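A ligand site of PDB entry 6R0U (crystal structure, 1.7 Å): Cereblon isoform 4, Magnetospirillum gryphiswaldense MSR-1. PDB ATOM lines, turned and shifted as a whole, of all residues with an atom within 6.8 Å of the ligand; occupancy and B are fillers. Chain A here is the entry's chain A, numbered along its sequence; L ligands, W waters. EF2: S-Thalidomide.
OG of Ser 79 sits at hydrogen-bond distance from O of Tyr 84, at 2.9 Å.
N of Trp 86 lies within hydrogen-bond range of O of Ser 75 (2.7 Å).
The side-chain hydroxyl (OG) of Ser 75 lies within hydrogen-bond range of the backbone NH (N) of Glu 77 (3.1 Å).
O of Phe 81 is in hydrogen-bond range of OG of Ser 79, at 3.0 Å.
NE1 of Trp 80 lies within hydrogen-bond range of O of Phe 50.
The backbone NH (N) of Met 55 lies within hydrogen-bond range of the side-chain amide oxygen (OD1) of Asn 51 (3.0 Å).
NE1 of Trp 86 sits at hydrogen-bond distance from O of Glu 77 (2.8 Å).
The side-chain amide oxygen (OD1) of Asn 51 lies within hydrogen-bond range of the backbone NH (N) of Ala 53, 3.1 Å away.
N of Trp 80 sits at hydrogen-bond distance from O05 of the ligand.
The backbone carbonyl oxygen (O) of Phe 78 lies within hydrogen-bond range of a nitrogen (N03) of the ligand, 2.9 Å away.
The side-chain hydroxyl (OH) of Tyr 102 lies within hydrogen-bond range of an oxygen (O05) of the ligand, 2.8 Å away.
The side-chain amide nitrogen (ND2) of Asn 51 is in hydrogen-bond range of an oxygen (O18) of the ligand (3.1 Å).
Water W2 bridges the indole nitrogen (NE1) of Trp 100 and an oxygen (O18) of the ligand.
Pro 52 touches the ligand (CD to O01, 3.4 Å).
Glu 77 touches the ligand.
CA of Ser 79 touches O05 of the ligand (3.5 Å).
Trp 86 touches the ligand.
NE1 of Trp 100 touches C07 of the ligand, at 3.4 Å.
Along chain A the residues within 4 Å of the ligand span positions 51 to 102.
The nearest printed residue that does not touch the ligand is Phe 57 (4.3 Å).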
ATOM      1  N   VAL A  49     -14.670  19.361  19.896  1.00  0.00           N
ATOM      2  CA  VAL A  49     -14.488  19.231  18.445  1.00  0.00           C
ATOM      3  C   VAL A  49     -13.021  19.390  18.071  1.00  0.00           C
ATOM      4  O   VAL A  49     -12.270  19.886  18.859  1.00  0.00           O
ATOM      5  CB  VAL A  49     -15.304  20.312  17.698  1.00  0.00           C
ATOM      6  CG1 VAL A  49     -16.797  20.124  18.000  1.00  0.00           C
ATOM      7  CG2 VAL A  49     -14.899  21.729  18.135  1.00  0.00           C
ATOM      8  N   PHE A  50     -12.663  18.919  16.860  1.00  0.00           N
ATOM      9  CA  PHE A  50     -11.347  19.019  16.330  1.00  0.00           C
ATOM     10  C   PHE A  50     -11.427  19.599  14.938  1.00  0.00           C
ATOM     11  O   PHE A  50     -12.331  19.270  14.163  1.00  0.00           O
ATOM     12  CB  PHE A  50     -10.602  17.554  16.345  1.00  0.00           C
ATOM     13  N   ASN A  51     -10.473  20.419  14.564  1.00  0.00           N
ATOM     14  CA  ASN A  51     -10.341  20.915  13.199  1.00  0.00           C
ATOM     15  C   ASN A  51      -9.375  20.046  12.340  1.00  0.00           C
ATOM     16  O   ASN A  51      -8.822  19.072  12.818  1.00  0.00           O
ATOM     17  CB  ASN A  51      -9.983  22.420  13.250  1.00  0.00           C
ATOM     18  CG  ASN A  51      -8.557  22.675  13.664  1.00  0.00           C
ATOM     19  OD1 ASN A  51      -7.742  21.763  13.787  1.00  0.00           O
ATOM     20  ND2 ASN A  51      -8.229  23.952  13.831  1.00  0.00           N
ATOM     21  N   PRO A  52      -9.226  20.374  11.058  1.00  0.00           N
ATOM     22  CA  PRO A  52      -8.398  19.508  10.191  1.00  0.00           C
ATOM     23  C   PRO A  52      -6.936  19.487  10.592  1.00  0.00           C
ATOM     24  O   PRO A  52      -6.292  18.517  10.260  1.00  0.00           O
ATOM     25  CB  PRO A  52      -8.576  20.116   8.796  1.00  0.00           C
ATOM     26  CG  PRO A  52      -9.976  20.757   8.842  1.00  0.00           C
ATOM     27  CD  PRO A  52     -10.044  21.326  10.252  1.00  0.00           C
ATOM     28  N   ALA A  53      -6.436  20.493  11.279  1.00  0.00           N
ATOM     29  CA  ALA A  53      -5.101  20.525  11.793  1.00  0.00           C
ATOM     30  C   ALA A  53      -4.989  19.726  13.100  1.00  0.00           C
ATOM     31  O   ALA A  53      -3.939  19.732  13.727  1.00  0.00           O
ATOM     32  CB  ALA A  53      -4.687  21.986  12.027  1.00  0.00           C
ATOM     33  N   MET A  55      -6.412  20.336  16.041  1.00  0.00           N
ATOM     34  CA  MET A  55      -6.587  21.102  17.286  1.00  0.00           C
ATOM     35  C   MET A  55      -7.931  20.712  17.885  1.00  0.00           C
ATOM     36  O   MET A  55      -8.948  20.722  17.178  1.00  0.00           O
ATOM     37  CB  MET A  55      -6.581  22.612  17.037  1.00  0.00           C
ATOM     38  CG  MET A  55      -5.348  23.144  16.347  1.00  0.00           C
ATOM     39  SD  MET A  55      -5.318  24.942  16.222  1.00  0.00           S
ATOM     40  CE  MET A  55      -5.598  25.180  14.473  1.00  0.00           C
ATOM     41  N   PHE A  57     -10.928  21.695  20.542  1.00  0.00           N
ATOM     42  CA  PHE A  57     -11.566  22.927  21.114  1.00  0.00           C
ATOM     43  C   PHE A  57     -12.743  22.428  21.950  1.00  0.00           C
ATOM     44  O   PHE A  57     -13.505  21.546  21.535  1.00  0.00           O
ATOM     45  CB  PHE A  57     -12.085  23.885  20.057  1.00  0.00           C
ATOM     46  CG  PHE A  57     -11.067  24.385  19.059  1.00  0.00           C
ATOM     47  CD1 PHE A  57     -10.243  25.439  19.347  1.00  0.00           C
ATOM     48  CD2 PHE A  57     -10.947  23.841  17.800  1.00  0.00           C
ATOM     49  CE1 PHE A  57      -9.271  25.890  18.446  1.00  0.00           C
ATOM     50  CE2 PHE A  57      -9.954  24.270  16.919  1.00  0.00           C
ATOM     51  CZ  PHE A  57      -9.144  25.319  17.233  1.00  0.00           C
ATOM     52  N   SER A  75     -18.626  29.797   5.332  1.00  0.00           N
ATOM     53  CA  SER A  75     -18.228  28.564   4.664  1.00  0.00           C
ATOM     54  C   SER A  75     -18.906  27.399   5.347  1.00  0.00           C
ATOM     55  O   SER A  75     -18.979  27.377   6.580  1.00  0.00           O
ATOM     56  CB  SER A  75     -16.725  28.364   4.746  1.00  0.00           C
ATOM     57  OG  SER A  75     -16.361  27.105   4.118  1.00  0.00           O
ATOM     58  N   GLU A  77     -17.570  24.296   4.807  1.00  0.00           N
ATOM     59  CA  GLU A  77     -16.485  23.287   4.846  1.00  0.00           C
ATOM     60  C   GLU A  77     -16.163  22.879   6.316  1.00  0.00           C
ATOM     61  O   GLU A  77     -15.975  23.740   7.167  1.00  0.00           O
ATOM     62  CB  GLU A  77     -15.194  23.806   4.178  1.00  0.00           C
ATOM     63  CG  GLU A  77     -14.533  22.769   3.247  1.00  0.00           C
ATOM     64  CD  GLU A  77     -13.057  23.010   2.876  1.00  0.00           C
ATOM     65  OE1 GLU A  77     -12.476  24.079   3.207  1.00  0.00           O
ATOM     66  OE2 GLU A  77     -12.488  22.095   2.232  1.00  0.00           O
ATOM     67  N   PHE A  78     -16.213  21.600   6.600  1.00  0.00           N
ATOM     68  CA  PHE A  78     -15.873  21.012   7.910  1.00  0.00           C
ATOM     69  C   PHE A  78     -16.749  21.491   9.076  1.00  0.00           C
ATOM     70  O   PHE A  78     -16.299  21.448  10.203  1.00  0.00           O
ATOM     71  CB  PHE A  78     -14.390  21.269   8.282  1.00  0.00           C
ATOM     72  CG  PHE A  78     -13.423  20.909   7.225  1.00  0.00           C
ATOM     73  CD1 PHE A  78     -13.245  19.608   6.887  1.00  0.00           C
ATOM     74  CD2 PHE A  78     -12.728  21.891   6.531  1.00  0.00           C
ATOM     75  CE1 PHE A  78     -12.367  19.230   5.928  1.00  0.00           C
ATOM     76  CE2 PHE A  78     -11.792  21.524   5.570  1.00  0.00           C
ATOM     77  CZ  PHE A  78     -11.610  20.183   5.274  1.00  0.00           C
ATOM     78  N   SER A  79     -17.943  22.028   8.824  1.00  0.00           N
ATOM     79  CA  SER A  79     -18.752  22.525   9.896  1.00  0.00           C
ATOM     80  C   SER A  79     -19.052  21.483  10.889  1.00  0.00           C
ATOM     81  O   SER A  79     -19.510  20.458  10.555  1.00  0.00           O
ATOM     82  CB  SER A  79     -20.060  23.142   9.415  1.00  0.00           C
ATOM     83  OG  SER A  79     -20.779  23.739  10.493  1.00  0.00           O
ATOM     84  N   TRP A  80     -18.830  21.827  12.152  1.00  0.00           N
ATOM     85  CA  TRP A  80     -19.141  21.010  13.281  1.00  0.00           C
ATOM     86  C   TRP A  80     -20.620  20.946  13.576  1.00  0.00           C
ATOM     87  O   TRP A  80     -21.042  20.144  14.385  1.00  0.00           O
ATOM     88  CB  TRP A  80     -18.397  21.454  14.501  1.00  0.00           C
ATOM     89  CG  TRP A  80     -16.927  21.355  14.390  1.00  0.00           C
ATOM     90  CD1 TRP A  80     -16.185  20.315  13.957  1.00  0.00           C
ATOM     91  CD2 TRP A  80     -16.009  22.394  14.787  1.00  0.00           C
ATOM     92  NE1 TRP A  80     -14.845  20.624  14.051  1.00  0.00           N
ATOM     93  CE2 TRP A  80     -14.699  21.881  14.575  1.00  0.00           C
ATOM     94  CE3 TRP A  80     -16.167  23.670  15.315  1.00  0.00           C
ATOM     95  CZ2 TRP A  80     -13.585  22.621  14.862  1.00  0.00           C
ATOM     96  CZ3 TRP A  80     -15.073  24.412  15.592  1.00  0.00           C
ATOM     97  CH2 TRP A  80     -13.784  23.897  15.361  1.00  0.00           C
ATOM     98  N   PHE A  81     -21.438  21.784  12.939  1.00  0.00           N
ATOM     99  CA  PHE A  81     -22.855  21.841  13.301  1.00  0.00           C
ATOM    100  C   PHE A  81     -23.598  21.730  12.005  1.00  0.00           C
ATOM    101  O   PHE A  81     -23.522  22.628  11.154  1.00  0.00           O
ATOM    102  CB  PHE A  81     -23.134  23.168  13.986  1.00  0.00           C
ATOM    103  CG  PHE A  81     -22.431  23.318  15.301  1.00  0.00           C
ATOM    104  CD1 PHE A  81     -22.952  22.713  16.439  1.00  0.00           C
ATOM    105  CD2 PHE A  81     -21.313  24.064  15.405  1.00  0.00           C
ATOM    106  CE1 PHE A  81     -22.402  22.958  17.679  1.00  0.00           C
ATOM    107  CE2 PHE A  81     -20.704  24.268  16.659  1.00  0.00           C
ATOM    108  CZ  PHE A  81     -21.228  23.655  17.801  1.00  0.00           C
ATOM    109  N   TYR A  84     -25.098  24.483   9.211  1.00  0.00           N
ATOM    110  CA  TYR A  84     -24.614  25.817   9.444  1.00  0.00           C
ATOM    111  C   TYR A  84     -23.309  26.059   8.766  1.00  0.00           C
ATOM    112  O   TYR A  84     -22.468  25.141   8.654  1.00  0.00           O
ATOM    113  CB  TYR A  84     -24.410  26.069  10.923  1.00  0.00           C
ATOM    114  CG  TYR A  84     -25.662  26.024  11.755  1.00  0.00           C
ATOM    115  CD1 TYR A  84     -26.075  24.825  12.289  1.00  0.00           C
ATOM    116  CD2 TYR A  84     -26.428  27.168  12.004  1.00  0.00           C
ATOM    117  CE1 TYR A  84     -27.197  24.731  13.130  1.00  0.00           C
ATOM    118  CE2 TYR A  84     -27.535  27.130  12.782  1.00  0.00           C
ATOM    119  CZ  TYR A  84     -27.945  25.911  13.325  1.00  0.00           C
ATOM    120  OH  TYR A  84     -29.054  25.778  14.083  1.00  0.00           O
ATOM    121  N   TRP A  86     -19.996  28.722   8.736  1.00  0.00           N
ATOM    122  CA  TRP A  86     -19.220  29.445   9.779  1.00  0.00           C
ATOM    123  C   TRP A  86     -18.422  30.585   9.230  1.00  0.00           C
ATOM    124  O   TRP A  86     -17.966  30.584   8.065  1.00  0.00           O
ATOM    125  CB  TRP A  86     -18.307  28.520  10.572  1.00  0.00           C
ATOM    126  CG  TRP A  86     -17.368  27.704   9.769  1.00  0.00           C
ATOM    127  CD1 TRP A  86     -17.572  26.454   9.348  1.00  0.00           C
ATOM    128  CD2 TRP A  86     -16.093  28.120   9.232  1.00  0.00           C
ATOM    129  NE1 TRP A  86     -16.529  26.063   8.556  1.00  0.00           N
ATOM    130  CE2 TRP A  86     -15.594  27.058   8.490  1.00  0.00           C
ATOM    131  CE3 TRP A  86     -15.323  29.307   9.325  1.00  0.00           C
ATOM    132  CZ2 TRP A  86     -14.355  27.101   7.841  1.00  0.00           C
ATOM    133  CZ3 TRP A  86     -14.096  29.354   8.720  1.00  0.00           C
ATOM    134  CH2 TRP A  86     -13.612  28.222   7.970  1.00  0.00           C
ATOM    135  N   THR A  87     -18.208  31.551  10.116  1.00  0.00           N
ATOM    136  CA  THR A  87     -17.221  32.627   9.880  1.00  0.00           C
ATOM    137  C   THR A  87     -16.384  32.698  11.151  1.00  0.00           C
ATOM    138  O   THR A  87     -16.873  32.510  12.234  1.00  0.00           O
ATOM    139  CB  THR A  87     -17.813  33.999   9.635  1.00  0.00           C
ATOM    140  OG1 THR A  87     -18.755  34.335  10.667  1.00  0.00           O
ATOM    141  CG2 THR A  87     -18.465  34.111   8.240  1.00  0.00           C
ATOM    142  N   ILE A  88     -15.129  33.014  10.970  1.00  0.00           N
ATOM    143  CA  ILE A  88     -14.203  33.212  12.100  1.00  0.00           C
ATOM    144  C   ILE A  88     -14.613  34.436  12.897  1.00  0.00           C
ATOM    145  O   ILE A  88     -14.925  35.519  12.292  1.00  0.00           O
ATOM    146  CB  ILE A  88     -12.763  33.356  11.568  1.00  0.00           C
ATOM    147  CG1 ILE A  88     -12.308  31.964  11.074  1.00  0.00           C
ATOM    148  CG2 ILE A  88     -11.799  33.851  12.669  1.00  0.00           C
ATOM    149  CD1 ILE A  88     -11.036  32.088  10.224  1.00  0.00           C
ATOM    150  N   HIS A  97      -8.415  34.979  18.374  1.00  0.00           N
ATOM    151  CA  HIS A  97      -9.415  34.143  17.774  1.00  0.00           C
ATOM    152  C   HIS A  97     -10.269  33.500  18.879  1.00  0.00           C
ATOM    153  O   HIS A  97      -9.809  32.634  19.595  1.00  0.00           O
ATOM    154  CB  HIS A  97      -8.755  33.063  16.943  1.00  0.00           C
ATOM    155  CG  HIS A  97      -9.771  32.080  16.395  1.00  0.00           C
ATOM    156  ND1 HIS A  97      -9.417  30.784  16.022  1.00  0.00           N
ATOM    157  CD2 HIS A  97     -11.077  32.249  16.092  1.00  0.00           C
ATOM    158  CE1 HIS A  97     -10.522  30.184  15.597  1.00  0.00           C
ATOM    159  NE2 HIS A  97     -11.527  31.048  15.620  1.00  0.00           N
ATOM    160  N   TRP A 100     -16.267  31.095  16.465  1.00  0.00           N
ATOM    161  CA  TRP A 100     -16.919  31.188  15.124  1.00  0.00           C
ATOM    162  C   TRP A 100     -18.343  31.676  15.294  1.00  0.00           C
ATOM    163  O   TRP A 100     -18.972  31.450  16.334  1.00  0.00           O
ATOM    164  CB  TRP A 100     -16.899  29.805  14.452  1.00  0.00           C
ATOM    165  CG  TRP A 100     -15.526  29.236  14.272  1.00  0.00           C
ATOM    166  CD1 TRP A 100     -14.749  29.363  13.185  1.00  0.00           C
ATOM    167  CD2 TRP A 100     -14.776  28.506  15.234  1.00  0.00           C
ATOM    168  NE1 TRP A 100     -13.528  28.782  13.423  1.00  0.00           N
ATOM    169  CE2 TRP A 100     -13.544  28.198  14.648  1.00  0.00           C
ATOM    170  CE3 TRP A 100     -15.040  28.045  16.540  1.00  0.00           C
ATOM    171  CZ2 TRP A 100     -12.543  27.487  15.347  1.00  0.00           C
ATOM    172  CZ3 TRP A 100     -14.013  27.348  17.239  1.00  0.00           C
ATOM    173  CH2 TRP A 100     -12.801  27.100  16.637  1.00  0.00           C
ATOM    174  N   TYR A 102     -21.983  31.049  13.481  1.00  0.00           N
ATOM    175  CA  TYR A 102     -22.672  30.080  12.630  1.00  0.00           C
ATOM    176  C   TYR A 102     -23.963  30.710  12.118  1.00  0.00           C
ATOM    177  O   TYR A 102     -24.674  31.430  12.831  1.00  0.00           O
ATOM    178  CB  TYR A 102     -22.968  28.810  13.410  1.00  0.00           C
ATOM    179  CG  TYR A 102     -21.701  28.016  13.692  1.00  0.00           C
ATOM    180  CD1 TYR A 102     -21.200  27.144  12.720  1.00  0.00           C
ATOM    181  CD2 TYR A 102     -20.944  28.250  14.824  1.00  0.00           C
ATOM    182  CE1 TYR A 102     -20.007  26.482  12.922  1.00  0.00           C
ATOM    183  CE2 TYR A 102     -19.782  27.510  15.058  1.00  0.00           C
ATOM    184  CZ  TYR A 102     -19.275  26.712  14.093  1.00  0.00           C
ATOM    185  OH  TYR A 102     -18.106  26.030  14.375  1.00  0.00           O
HETATM  186  O01 EF2 L   1     -12.970  22.728  11.400  1.00  0.00           O
HETATM  187  C02 EF2 L   1     -13.714  23.620  11.671  1.00  0.00           C
HETATM  188  N03 EF2 L   1     -15.062  23.520  11.732  1.00  0.00           N
HETATM  189  C04 EF2 L   1     -15.886  24.576  12.043  1.00  0.00           C
HETATM  190  O05 EF2 L   1     -17.073  24.455  12.298  1.00  0.00           O
HETATM  191  C06 EF2 L   1     -15.283  25.918  12.292  1.00  0.00           C
HETATM  192  C07 EF2 L   1     -14.067  26.035  11.451  1.00  0.00           C
HETATM  193  C08 EF2 L   1     -13.132  24.965  11.932  1.00  0.00           C
HETATM  194  N09 EF2 L   1     -11.939  25.148  11.173  1.00  0.00           N
HETATM  195  C11 EF2 L   1      -8.432  25.571   8.148  1.00  0.00           C
HETATM  196  C12 EF2 L   1      -9.767  25.189   8.191  1.00  0.00           C
HETATM  197  C13 EF2 L   1     -10.406  25.231   9.447  1.00  0.00           C
HETATM  198  C14 EF2 L   1      -9.713  25.613  10.603  1.00  0.00           C
HETATM  199  O16 EF2 L   1     -12.775  24.517   9.035  1.00  0.00           O
HETATM  200  O18 EF2 L   1     -10.660  25.652  12.862  1.00  0.00           O
HETATM  201  C19 EF2 L   1      -8.366  25.972  10.570  1.00  0.00           C
HETATM  202  C20 EF2 L   1      -7.716  25.930   9.323  1.00  0.00           C
HETATM  203  C3  EF2 L   1     -10.773  25.520  11.649  1.00  0.00           C
HETATM  204  C4  EF2 L   1     -11.686  24.978   9.858  1.00  0.00           C
HETATM  205  O   HOH W   1      -9.267  27.801  13.808  1.00  0.00           O
HETATM  206  O   HOH W   2     -11.424  28.555  11.672  1.00  0.00           O
